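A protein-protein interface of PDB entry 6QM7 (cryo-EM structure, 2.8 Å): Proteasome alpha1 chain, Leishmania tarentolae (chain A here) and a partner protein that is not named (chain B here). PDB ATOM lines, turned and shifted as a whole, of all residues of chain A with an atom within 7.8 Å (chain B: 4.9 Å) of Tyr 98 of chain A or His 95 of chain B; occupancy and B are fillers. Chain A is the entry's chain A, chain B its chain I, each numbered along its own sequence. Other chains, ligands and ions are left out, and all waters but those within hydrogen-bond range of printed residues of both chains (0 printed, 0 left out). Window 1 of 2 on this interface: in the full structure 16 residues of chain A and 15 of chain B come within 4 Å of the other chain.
His 95 of chain B touches two residues of chain A.
Of the printed residues of chain B, Tyr 102 of chain A touches His 91, His 95 and Glu 107.
Of the printed residues of chain A, Glu 107 of chain B touches Tyr 102.
Printed residues of chain B within 4 Å of Arg 114 of chain A: Glu 98 (2.9 Å).
Of the printed residues of chain A, His 91 of chain B touches Tyr 102.
Printed residues of chain B within 4 Å of Val 110 of chain A: Thr 99 (3.5 Å).
Tyr 100 of chain A touches none of the printed residues of chain B.
Of the 20 printed residues of chain A, 4 touch a printed residue of chain B.
Hydrophobic or aromatic side chains of chain A within 4 Å of the printed part of chain B: Tyr 98, Tyr 102 and Val 110.
Of the 11 printed residues of chain B, 5 touch a printed residue of chain A.
Hydrophobic or aromatic side chains of chain B that line the printed part of chain A: His 91 and His 95.
Among the printed residues, 6 pairs touch across the chains.
Among the printed residues, Asp or Glu carboxylates within 4 Å of a Lys or Arg side-chain nitrogen of the other chain: Arg 114 of chain A with Glu 98 of chain B (2.9 Å).
The side-chain carboxylate (OE1) of Glu 94 of chain A lies within salt-bridge range of the guanidinium group (NH1) of Arg 114 of chain A (2.5 Å).
O of His 95 of chain B sits at hydrogen-bond distance from OG1 of Thr 99 of chain B, at 2.9 Å.
OE1 of Glu 107 of chain B lies within hydrogen-bond range of ND1 of His 95 of chain B (3.2 Å).
Among the printed residues, merely in contact across the chains: Tyr 102 of chain A with His 95 of chain B (3.8 Å), Tyr 102 of chain A with Glu 107 of chain B (3.3 Å) and Val 110 of chain A with Thr 99 of chain B (3.5 Å).
The side-chain hydroxyl (OH) of Tyr 98 of chain A is in hydrogen-bond range of a ring nitrogen (NE2) of His 95 of chain B (2.9 Å).
A ring nitrogen (NE2) of His 91 of chain B sits at hydrogen-bond distance from the side-chain hydroxyl (OH) of Tyr 102 of chain A (2.9 Å).
The guanidinium group of Arg 114 of chain A lies within salt-bridge range of the side-chain carboxylate of Glu 98 of chain B, at 2.9 Å.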
ATOM      1  N   ALA A  91     -16.167  15.061  15.111  1.00  0.00           N
ATOM      2  CA  ALA A  91     -14.918  14.333  14.777  1.00  0.00           C
ATOM      3  C   ALA A  91     -14.300  14.912  13.510  1.00  0.00           C
ATOM      4  O   ALA A  91     -13.088  15.111  13.475  1.00  0.00           O
ATOM      5  CB  ALA A  91     -15.190  12.866  14.597  1.00  0.00           C
ATOM      6  N   ARG A  92     -15.129  15.159  12.506  1.00  0.00           N
ATOM      7  CA  ARG A  92     -14.722  15.783  11.226  1.00  0.00           C
ATOM      8  C   ARG A  92     -14.212  17.199  11.487  1.00  0.00           C
ATOM      9  O   ARG A  92     -13.150  17.542  10.942  1.00  0.00           O
ATOM     10  CB  ARG A  92     -15.909  15.780  10.272  1.00  0.00           C
ATOM     11  CG  ARG A  92     -16.252  14.392   9.777  1.00  0.00           C
ATOM     12  CD  ARG A  92     -17.361  14.453   8.760  1.00  0.00           C
ATOM     13  NE  ARG A  92     -17.594  13.142   8.184  1.00  0.00           N
ATOM     14  CZ  ARG A  92     -18.684  12.791   7.520  1.00  0.00           C
ATOM     15  NH1 ARG A  92     -19.666  13.658   7.326  1.00  0.00           N
ATOM     16  NH2 ARG A  92     -18.798  11.562   7.056  1.00  0.00           N
ATOM     17  N   GLU A  93     -14.961  17.986  12.265  1.00  0.00           N
ATOM     18  CA  GLU A  93     -14.560  19.341  12.729  1.00  0.00           C
ATOM     19  C   GLU A  93     -13.171  19.218  13.362  1.00  0.00           C
ATOM     20  O   GLU A  93     -12.253  19.926  12.912  1.00  0.00           O
ATOM     21  CB  GLU A  93     -15.567  19.902  13.737  1.00  0.00           C
ATOM     22  CG  GLU A  93     -15.993  21.341  13.482  1.00  0.00           C
ATOM     23  CD  GLU A  93     -17.108  21.861  14.394  1.00  0.00           C
ATOM     24  OE1 GLU A  93     -18.035  21.078  14.739  1.00  0.00           O
ATOM     25  OE2 GLU A  93     -17.055  23.058  14.765  1.00  0.00           O
ATOM     26  N   GLU A  94     -13.032  18.303  14.325  1.00  0.00           N
ATOM     27  CA  GLU A  94     -11.820  18.107  15.167  1.00  0.00           C
ATOM     28  C   GLU A  94     -10.620  17.737  14.290  1.00  0.00           C
ATOM     29  O   GLU A  94      -9.514  18.197  14.598  1.00  0.00           O
ATOM     30  CB  GLU A  94     -12.076  17.017  16.213  1.00  0.00           C
ATOM     31  CG  GLU A  94     -11.000  16.920  17.276  1.00  0.00           C
ATOM     32  CD  GLU A  94     -10.760  18.198  18.075  1.00  0.00           C
ATOM     33  OE1 GLU A  94      -9.581  18.524  18.333  1.00  0.00           O
ATOM     34  OE2 GLU A  94     -11.750  18.874  18.430  1.00  0.00           O
ATOM     35  N   ALA A  95     -10.857  16.929  13.254  1.00  0.00           N
ATOM     36  CA  ALA A  95      -9.849  16.390  12.312  1.00  0.00           C
ATOM     37  C   ALA A  95      -9.424  17.467  11.318  1.00  0.00           C
ATOM     38  O   ALA A  95      -8.225  17.593  11.073  1.00  0.00           O
ATOM     39  CB  ALA A  95     -10.414  15.192  11.591  1.00  0.00           C
ATOM     40  N   SER A  96     -10.388  18.174  10.738  1.00  0.00           N
ATOM     41  CA  SER A  96     -10.169  19.333   9.833  1.00  0.00           C
ATOM     42  C   SER A  96      -9.301  20.353  10.563  1.00  0.00           C
ATOM     43  O   SER A  96      -8.281  20.759  10.006  1.00  0.00           O
ATOM     44  CB  SER A  96     -11.484  19.959   9.410  1.00  0.00           C
ATOM     45  OG  SER A  96     -12.369  18.989   8.854  1.00  0.00           O
ATOM     46  N   ASP A  97      -9.720  20.701  11.782  1.00  0.00           N
ATOM     47  CA  ASP A  97      -9.103  21.718  12.670  1.00  0.00           C
ATOM     48  C   ASP A  97      -7.665  21.317  12.975  1.00  0.00           C
ATOM     49  O   ASP A  97      -6.806  22.196  13.017  1.00  0.00           O
ATOM     50  CB  ASP A  97      -9.881  21.849  13.983  1.00  0.00           C
ATOM     51  CG  ASP A  97      -9.940  23.265  14.532  1.00  0.00           C
ATOM     52  OD1 ASP A  97      -8.869  23.791  14.945  1.00  0.00           O
ATOM     53  OD2 ASP A  97     -11.064  23.839  14.544  1.00  0.00           O
ATOM     54  N   TYR A  98      -7.435  20.036  13.210  1.00  0.00           N
ATOM     55  CA  TYR A  98      -6.110  19.477  13.555  1.00  0.00           C
ATOM     56  C   TYR A  98      -5.198  19.580  12.331  1.00  0.00           C
ATOM     57  O   TYR A  98      -4.068  20.051  12.472  1.00  0.00           O
ATOM     58  CB  TYR A  98      -6.285  18.048  14.070  1.00  0.00           C
ATOM     59  CG  TYR A  98      -5.022  17.347  14.487  1.00  0.00           C
ATOM     60  CD1 TYR A  98      -4.734  17.112  15.827  1.00  0.00           C
ATOM     61  CD2 TYR A  98      -4.104  16.919  13.542  1.00  0.00           C
ATOM     62  CE1 TYR A  98      -3.566  16.460  16.217  1.00  0.00           C
ATOM     63  CE2 TYR A  98      -2.943  16.263  13.914  1.00  0.00           C
ATOM     64  CZ  TYR A  98      -2.666  16.029  15.254  1.00  0.00           C
ATOM     65  OH  TYR A  98      -1.524  15.353  15.585  1.00  0.00           O
ATOM     66  N   GLN A  99      -5.684  19.144  11.167  1.00  0.00           N
ATOM     67  CA  GLN A  99      -4.946  19.166   9.873  1.00  0.00           C
ATOM     68  C   GLN A  99      -4.559  20.617   9.585  1.00  0.00           C
ATOM     69  O   GLN A  99      -3.451  20.843   9.069  1.00  0.00           O
ATOM     70  CB  GLN A  99      -5.772  18.471   8.780  1.00  0.00           C
ATOM     71  CG  GLN A  99      -5.500  18.921   7.343  1.00  0.00           C
ATOM     72  CD  GLN A  99      -4.422  18.117   6.658  1.00  0.00           C
ATOM     73  OE1 GLN A  99      -4.566  16.913   6.431  1.00  0.00           O
ATOM     74  NE2 GLN A  99      -3.328  18.785   6.322  1.00  0.00           N
ATOM     75  N   TYR A 100      -5.413  21.576   9.917  1.00  0.00           N
ATOM     76  CA  TYR A 100      -5.111  22.998   9.644  1.00  0.00           C
ATOM     77  C   TYR A 100      -4.047  23.497  10.618  1.00  0.00           C
ATOM     78  O   TYR A 100      -3.123  24.201  10.183  1.00  0.00           O
ATOM     79  CB  TYR A 100      -6.348  23.886   9.705  1.00  0.00           C
ATOM     80  CG  TYR A 100      -6.001  25.305   9.346  1.00  0.00           C
ATOM     81  CD1 TYR A 100      -5.550  25.618   8.067  1.00  0.00           C
ATOM     82  CD2 TYR A 100      -6.021  26.316  10.296  1.00  0.00           C
ATOM     83  CE1 TYR A 100      -5.182  26.909   7.725  1.00  0.00           C
ATOM     84  CE2 TYR A 100      -5.658  27.612   9.963  1.00  0.00           C
ATOM     85  CZ  TYR A 100      -5.244  27.910   8.675  1.00  0.00           C
ATOM     86  OH  TYR A 100      -4.882  29.181   8.351  1.00  0.00           O
ATOM     87  N   ARG A 101      -4.182  23.142  11.890  1.00  0.00           N
ATOM     88  CA  ARG A 101      -3.308  23.635  12.980  1.00  0.00           C
ATOM     89  C   ARG A 101      -1.913  23.024  12.821  1.00  0.00           C
ATOM     90  O   ARG A 101      -0.955  23.776  13.043  1.00  0.00           O
ATOM     91  CB  ARG A 101      -3.950  23.366  14.350  1.00  0.00           C
ATOM     92  CG  ARG A 101      -3.034  23.629  15.540  1.00  0.00           C
ATOM     93  CD  ARG A 101      -3.706  23.536  16.900  1.00  0.00           C
ATOM     94  NE  ARG A 101      -4.449  24.753  17.226  1.00  0.00           N
ATOM     95  CZ  ARG A 101      -5.745  24.989  16.980  1.00  0.00           C
ATOM     96  NH1 ARG A 101      -6.521  24.083  16.401  1.00  0.00           N
ATOM     97  NH2 ARG A 101      -6.271  26.152  17.329  1.00  0.00           N
ATOM     98  N   TYR A 102      -1.802  21.737  12.477  1.00  0.00           N
ATOM     99  CA  TYR A 102      -0.528  20.960  12.491  1.00  0.00           C
ATOM    100  C   TYR A 102      -0.084  20.500  11.094  1.00  0.00           C
ATOM    101  O   TYR A 102       1.057  20.029  10.976  1.00  0.00           O
ATOM    102  CB  TYR A 102      -0.649  19.715  13.369  1.00  0.00           C
ATOM    103  CG  TYR A 102      -1.016  20.002  14.799  1.00  0.00           C
ATOM    104  CD1 TYR A 102      -0.114  20.593  15.673  1.00  0.00           C
ATOM    105  CD2 TYR A 102      -2.273  19.684  15.286  1.00  0.00           C
ATOM    106  CE1 TYR A 102      -0.456  20.851  16.997  1.00  0.00           C
ATOM    107  CE2 TYR A 102      -2.634  19.948  16.599  1.00  0.00           C
ATOM    108  CZ  TYR A 102      -1.720  20.524  17.460  1.00  0.00           C
ATOM    109  OH  TYR A 102      -2.082  20.760  18.750  1.00  0.00           O
ATOM    110  N   GLY A 103      -0.941  20.583  10.078  1.00  0.00           N
ATOM    111  CA  GLY A 103      -0.561  20.271   8.689  1.00  0.00           C
ATOM    112  C   GLY A 103      -0.362  18.787   8.447  1.00  0.00           C
ATOM    113  O   GLY A 103       0.292  18.445   7.437  1.00  0.00           O
ATOM    114  N   VAL A 104      -0.889  17.932   9.324  1.00  0.00           N
ATOM    115  CA  VAL A 104      -0.863  16.453   9.144  1.00  0.00           C
ATOM    116  C   VAL A 104      -2.236  15.918   9.530  1.00  0.00           C
ATOM    117  O   VAL A 104      -2.923  16.597  10.291  1.00  0.00           O
ATOM    118  CB  VAL A 104       0.266  15.783   9.948  1.00  0.00           C
ATOM    119  CG1 VAL A 104       1.633  16.326   9.560  1.00  0.00           C
ATOM    120  CG2 VAL A 104       0.063  15.897  11.450  1.00  0.00           C
ATOM    121  N   GLU A 105      -2.613  14.758   8.987  1.00  0.00           N
ATOM    122  CA  GLU A 105      -3.863  14.046   9.346  1.00  0.00           C
ATOM    123  C   GLU A 105      -3.835  13.753  10.847  1.00  0.00           C
ATOM    124  O   GLU A 105      -2.777  13.333  11.353  1.00  0.00           O
ATOM    125  CB  GLU A 105      -4.027  12.748   8.552  1.00  0.00           C
ATOM    126  CG  GLU A 105      -4.655  12.939   7.175  1.00  0.00           C
ATOM    127  CD  GLU A 105      -5.739  11.939   6.776  1.00  0.00           C
ATOM    128  OE1 GLU A 105      -6.437  11.404   7.676  1.00  0.00           O
ATOM    129  OE2 GLU A 105      -5.906  11.706   5.555  1.00  0.00           O
ATOM    130  N   ILE A 106      -4.962  13.967  11.522  1.00  0.00           N
ATOM    131  CA  ILE A 106      -5.122  13.623  12.960  1.00  0.00           C
ATOM    132  C   ILE A 106      -4.901  12.121  13.124  1.00  0.00           C
ATOM    133  O   ILE A 106      -5.537  11.325  12.440  1.00  0.00           O
ATOM    134  CB  ILE A 106      -6.479  14.101  13.520  1.00  0.00           C
ATOM    135  CG1 ILE A 106      -6.490  13.999  15.048  1.00  0.00           C
ATOM    136  CG2 ILE A 106      -7.661  13.375  12.891  1.00  0.00           C
ATOM    137  CD1 ILE A 106      -7.534  14.847  15.701  1.00  0.00           C
ATOM    138  N   PRO A 107      -3.939  11.692  13.971  1.00  0.00           N
ATOM    139  CA  PRO A 107      -3.801  10.292  14.347  1.00  0.00           C
ATOM    140  C   PRO A 107      -5.077   9.782  15.010  1.00  0.00           C
ATOM    141  O   PRO A 107      -5.625  10.499  15.791  1.00  0.00           O
ATOM    142  CB  PRO A 107      -2.688  10.272  15.401  1.00  0.00           C
ATOM    143  CG  PRO A 107      -1.910  11.517  15.124  1.00  0.00           C
ATOM    144  CD  PRO A 107      -2.917  12.525  14.614  1.00  0.00           C
ATOM    145  N   VAL A 110      -5.355  10.139  18.799  1.00  0.00           N
ATOM    146  CA  VAL A 110      -5.579  11.556  19.202  1.00  0.00           C
ATOM    147  C   VAL A 110      -7.051  11.890  18.990  1.00  0.00           C
ATOM    148  O   VAL A 110      -7.661  12.388  19.927  1.00  0.00           O
ATOM    149  CB  VAL A 110      -4.693  12.532  18.413  1.00  0.00           C
ATOM    150  CG1 VAL A 110      -5.055  13.983  18.690  1.00  0.00           C
ATOM    151  CG2 VAL A 110      -3.225  12.290  18.700  1.00  0.00           C
ATOM    152  N   LEU A 111      -7.573  11.654  17.788  1.00  0.00           N
ATOM    153  CA  LEU A 111      -8.990  11.918  17.448  1.00  0.00           C
ATOM    154  C   LEU A 111      -9.856  11.289  18.525  1.00  0.00           C
ATOM    155  O   LEU A 111     -10.712  11.987  19.043  1.00  0.00           O
ATOM    156  CB  LEU A 111      -9.366  11.317  16.090  1.00  0.00           C
ATOM    157  CG  LEU A 111     -10.853  11.458  15.759  1.00  0.00           C
ATOM    158  CD1 LEU A 111     -11.190  12.917  15.486  1.00  0.00           C
ATOM    159  CD2 LEU A 111     -11.258  10.578  14.593  1.00  0.00           C
ATOM    160  N   ARG A 114      -9.607  13.122  21.842  1.00  0.00           N
ATOM    161  CA  ARG A 114     -10.314  14.433  21.734  1.00  0.00           C
ATOM    162  C   ARG A 114     -11.827  14.210  21.804  1.00  0.00           C
ATOM    163  O   ARG A 114     -12.519  15.082  22.321  1.00  0.00           O
ATOM    164  CB  ARG A 114     -10.076  15.188  20.421  1.00  0.00           C
ATOM    165  CG  ARG A 114      -8.631  15.531  20.109  1.00  0.00           C
ATOM    166  CD  ARG A 114      -8.191  16.813  20.757  1.00  0.00           C
ATOM    167  NE  ARG A 114      -6.786  17.106  20.478  1.00  0.00           N
ATOM    168  CZ  ARG A 114      -6.309  17.750  19.415  1.00  0.00           C
ATOM    169  NH1 ARG A 114      -7.112  18.171  18.456  1.00  0.00           N
ATOM    170  NH2 ARG A 114      -5.008  17.963  19.311  1.00  0.00           N
ATOM    171  N   HIS B  91       4.519  23.806  22.595  1.00  0.00           N
ATOM    172  CA  HIS B  91       3.315  23.210  21.964  1.00  0.00           C
ATOM    173  C   HIS B  91       3.650  21.798  21.478  1.00  0.00           C
ATOM    174  O   HIS B  91       2.895  20.878  21.786  1.00  0.00           O
ATOM    175  CB  HIS B  91       2.782  24.101  20.837  1.00  0.00           C
ATOM    176  CG  HIS B  91       1.403  23.742  20.406  1.00  0.00           C
ATOM    177  ND1 HIS B  91       0.703  24.515  19.499  1.00  0.00           N
ATOM    178  CD2 HIS B  91       0.585  22.721  20.758  1.00  0.00           C
ATOM    179  CE1 HIS B  91      -0.485  23.974  19.296  1.00  0.00           C
ATOM    180  NE2 HIS B  91      -0.578  22.869  20.061  1.00  0.00           N
ATOM    181  N   LEU B  92       4.758  21.623  20.772  1.00  0.00           N
ATOM    182  CA  LEU B  92       5.185  20.289  20.288  1.00  0.00           C
ATOM    183  C   LEU B  92       5.325  19.323  21.461  1.00  0.00           C
ATOM    184  O   LEU B  92       4.917  18.167  21.283  1.00  0.00           O
ATOM    185  CB  LEU B  92       6.511  20.396  19.538  1.00  0.00           C
ATOM    186  CG  LEU B  92       6.436  21.090  18.183  1.00  0.00           C
ATOM    187  CD1 LEU B  92       7.804  21.063  17.515  1.00  0.00           C
ATOM    188  CD2 LEU B  92       5.374  20.460  17.293  1.00  0.00           C
ATOM    189  N   ALA B  93       5.904  19.768  22.578  1.00  0.00           N
ATOM    190  CA  ALA B  93       6.199  18.955  23.780  1.00  0.00           C
ATOM    191  C   ALA B  93       4.902  18.480  24.434  1.00  0.00           C
ATOM    192  O   ALA B  93       4.856  17.334  24.932  1.00  0.00           O
ATOM    193  CB  ALA B  93       6.995  19.774  24.756  1.00  0.00           C
ATOM    194  N   LEU B  94       3.922  19.376  24.460  1.00  0.00           N
ATOM    195  CA  LEU B  94       2.564  19.179  25.014  1.00  0.00           C
ATOM    196  C   LEU B  94       1.805  18.201  24.118  1.00  0.00           C
ATOM    197  O   LEU B  94       1.074  17.347  24.652  1.00  0.00           O
ATOM    198  CB  LEU B  94       1.857  20.539  25.040  1.00  0.00           C
ATOM    199  CG  LEU B  94       1.126  20.880  26.328  1.00  0.00           C
ATOM    200  CD1 LEU B  94       0.552  22.282  26.222  1.00  0.00           C
ATOM    201  CD2 LEU B  94       0.032  19.853  26.612  1.00  0.00           C
ATOM    202  N   HIS B  95       1.970  18.365  22.804  1.00  0.00           N
ATOM    203  CA  HIS B  95       1.332  17.568  21.725  1.00  0.00           C
ATOM    204  C   HIS B  95       1.928  16.165  21.679  1.00  0.00           C
ATOM    205  O   HIS B  95       1.239  15.248  21.236  1.00  0.00           O
ATOM    206  CB  HIS B  95       1.515  18.284  20.387  1.00  0.00           C
ATOM    207  CG  HIS B  95       0.747  17.657  19.281  1.00  0.00           C
ATOM    208  ND1 HIS B  95       1.362  17.252  18.114  1.00  0.00           N
ATOM    209  CD2 HIS B  95      -0.564  17.348  19.175  1.00  0.00           C
ATOM    210  CE1 HIS B  95       0.462  16.721  17.321  1.00  0.00           C
ATOM    211  NE2 HIS B  95      -0.737  16.764  17.953  1.00  0.00           N
ATOM    212  N   ARG B  96       3.179  16.037  22.094  1.00  0.00           N
ATOM    213  CA  ARG B  96       3.957  14.775  22.121  1.00  0.00           C
ATOM    214  C   ARG B  96       3.432  13.878  23.250  1.00  0.00           C
ATOM    215  O   ARG B  96       3.582  12.656  23.142  1.00  0.00           O
ATOM    216  CB  ARG B  96       5.435  15.147  22.290  1.00  0.00           C
ATOM    217  CG  ARG B  96       6.428  14.081  21.862  1.00  0.00           C
ATOM    218  CD  ARG B  96       7.721  14.685  21.360  1.00  0.00           C
ATOM    219  NE  ARG B  96       8.405  15.407  22.421  1.00  0.00           N
ATOM    220  CZ  ARG B  96       8.722  16.700  22.408  1.00  0.00           C
ATOM    221  NH1 ARG B  96       8.434  17.479  21.373  1.00  0.00           N
ATOM    222  NH2 ARG B  96       9.329  17.224  23.460  1.00  0.00           N
ATOM    223  N   LEU B  97       2.887  14.474  24.312  1.00  0.00           N
ATOM    224  CA  LEU B  97       2.267  13.750  25.449  1.00  0.00           C
ATOM    225  C   LEU B  97       0.857  13.302  25.063  1.00  0.00           C
ATOM    226  O   LEU B  97       0.397  12.285  25.601  1.00  0.00           O
ATOM    227  CB  LEU B  97       2.221  14.678  26.665  1.00  0.00           C
ATOM    228  CG  LEU B  97       3.578  15.096  27.218  1.00  0.00           C
ATOM    229  CD1 LEU B  97       3.444  16.152  28.301  1.00  0.00           C
ATOM    230  CD2 LEU B  97       4.332  13.890  27.744  1.00  0.00           C
ATOM    231  N   GLU B  98       0.188  14.068  24.207  1.00  0.00           N
ATOM    232  CA  GLU B  98      -1.172  13.759  23.711  1.00  0.00           C
ATOM    233  C   GLU B  98      -1.099  12.590  22.718  1.00  0.00           C
ATOM    234  O   GLU B  98      -1.932  11.669  22.828  1.00  0.00           O
ATOM    235  CB  GLU B  98      -1.784  15.018  23.095  1.00  0.00           C
ATOM    236  CG  GLU B  98      -3.225  14.824  22.637  1.00  0.00           C
ATOM    237  CD  GLU B  98      -3.949  16.095  22.229  1.00  0.00           C
ATOM    238  OE1 GLU B  98      -3.345  16.914  21.485  1.00  0.00           O
ATOM    239  OE2 GLU B  98      -5.123  16.259  22.640  1.00  0.00           O
ATOM    240  N   THR B  99      -0.140  12.634  21.791  1.00  0.00           N
ATOM    241  CA  THR B  99       0.027  11.667  20.673  1.00  0.00           C
ATOM    242  C   THR B  99       0.769  10.417  21.161  1.00  0.00           C
ATOM    243  O   THR B  99       0.452   9.323  20.663  1.00  0.00           O
ATOM    244  CB  THR B  99       0.761  12.313  19.489  1.00  0.00           C
ATOM    245  OG1 THR B  99       2.052  12.746  19.915  1.00  0.00           O
ATOM    246  CG2 THR B  99       0.038  13.498  18.886  1.00  0.00           C
ATOM    247  N   GLY B 100       1.709  10.570  22.094  1.00  0.00           N
ATOM    248  CA  GLY B 100       2.675   9.523  22.482  1.00  0.00           C
ATOM    249  C   GLY B 100       3.625   9.191  21.340  1.00  0.00           C
ATOM    250  O   GLY B 100       4.066   8.029  21.251  1.00  0.00           O
ATOM    251  N   GLU B 107       4.718  19.245  11.534  1.00  0.00           N
ATOM    252  CA  GLU B 107       3.906  19.818  12.644  1.00  0.00           C
ATOM    253  C   GLU B 107       4.607  21.080  13.145  1.00  0.00           C
ATOM    254  O   GLU B 107       3.943  22.102  13.283  1.00  0.00           O
ATOM    255  CB  GLU B 107       3.758  18.880  13.839  1.00  0.00           C
ATOM    256  CG  GLU B 107       3.046  17.563  13.565  1.00  0.00           C
ATOM    257  CD  GLU B 107       3.108  16.562  14.723  1.00  0.00           C
ATOM    258  OE1 GLU B 107       3.603  16.934  15.820  1.00  0.00           O
ATOM    259  OE2 GLU B 107       2.666  15.401  14.533  1.00  0.00           O
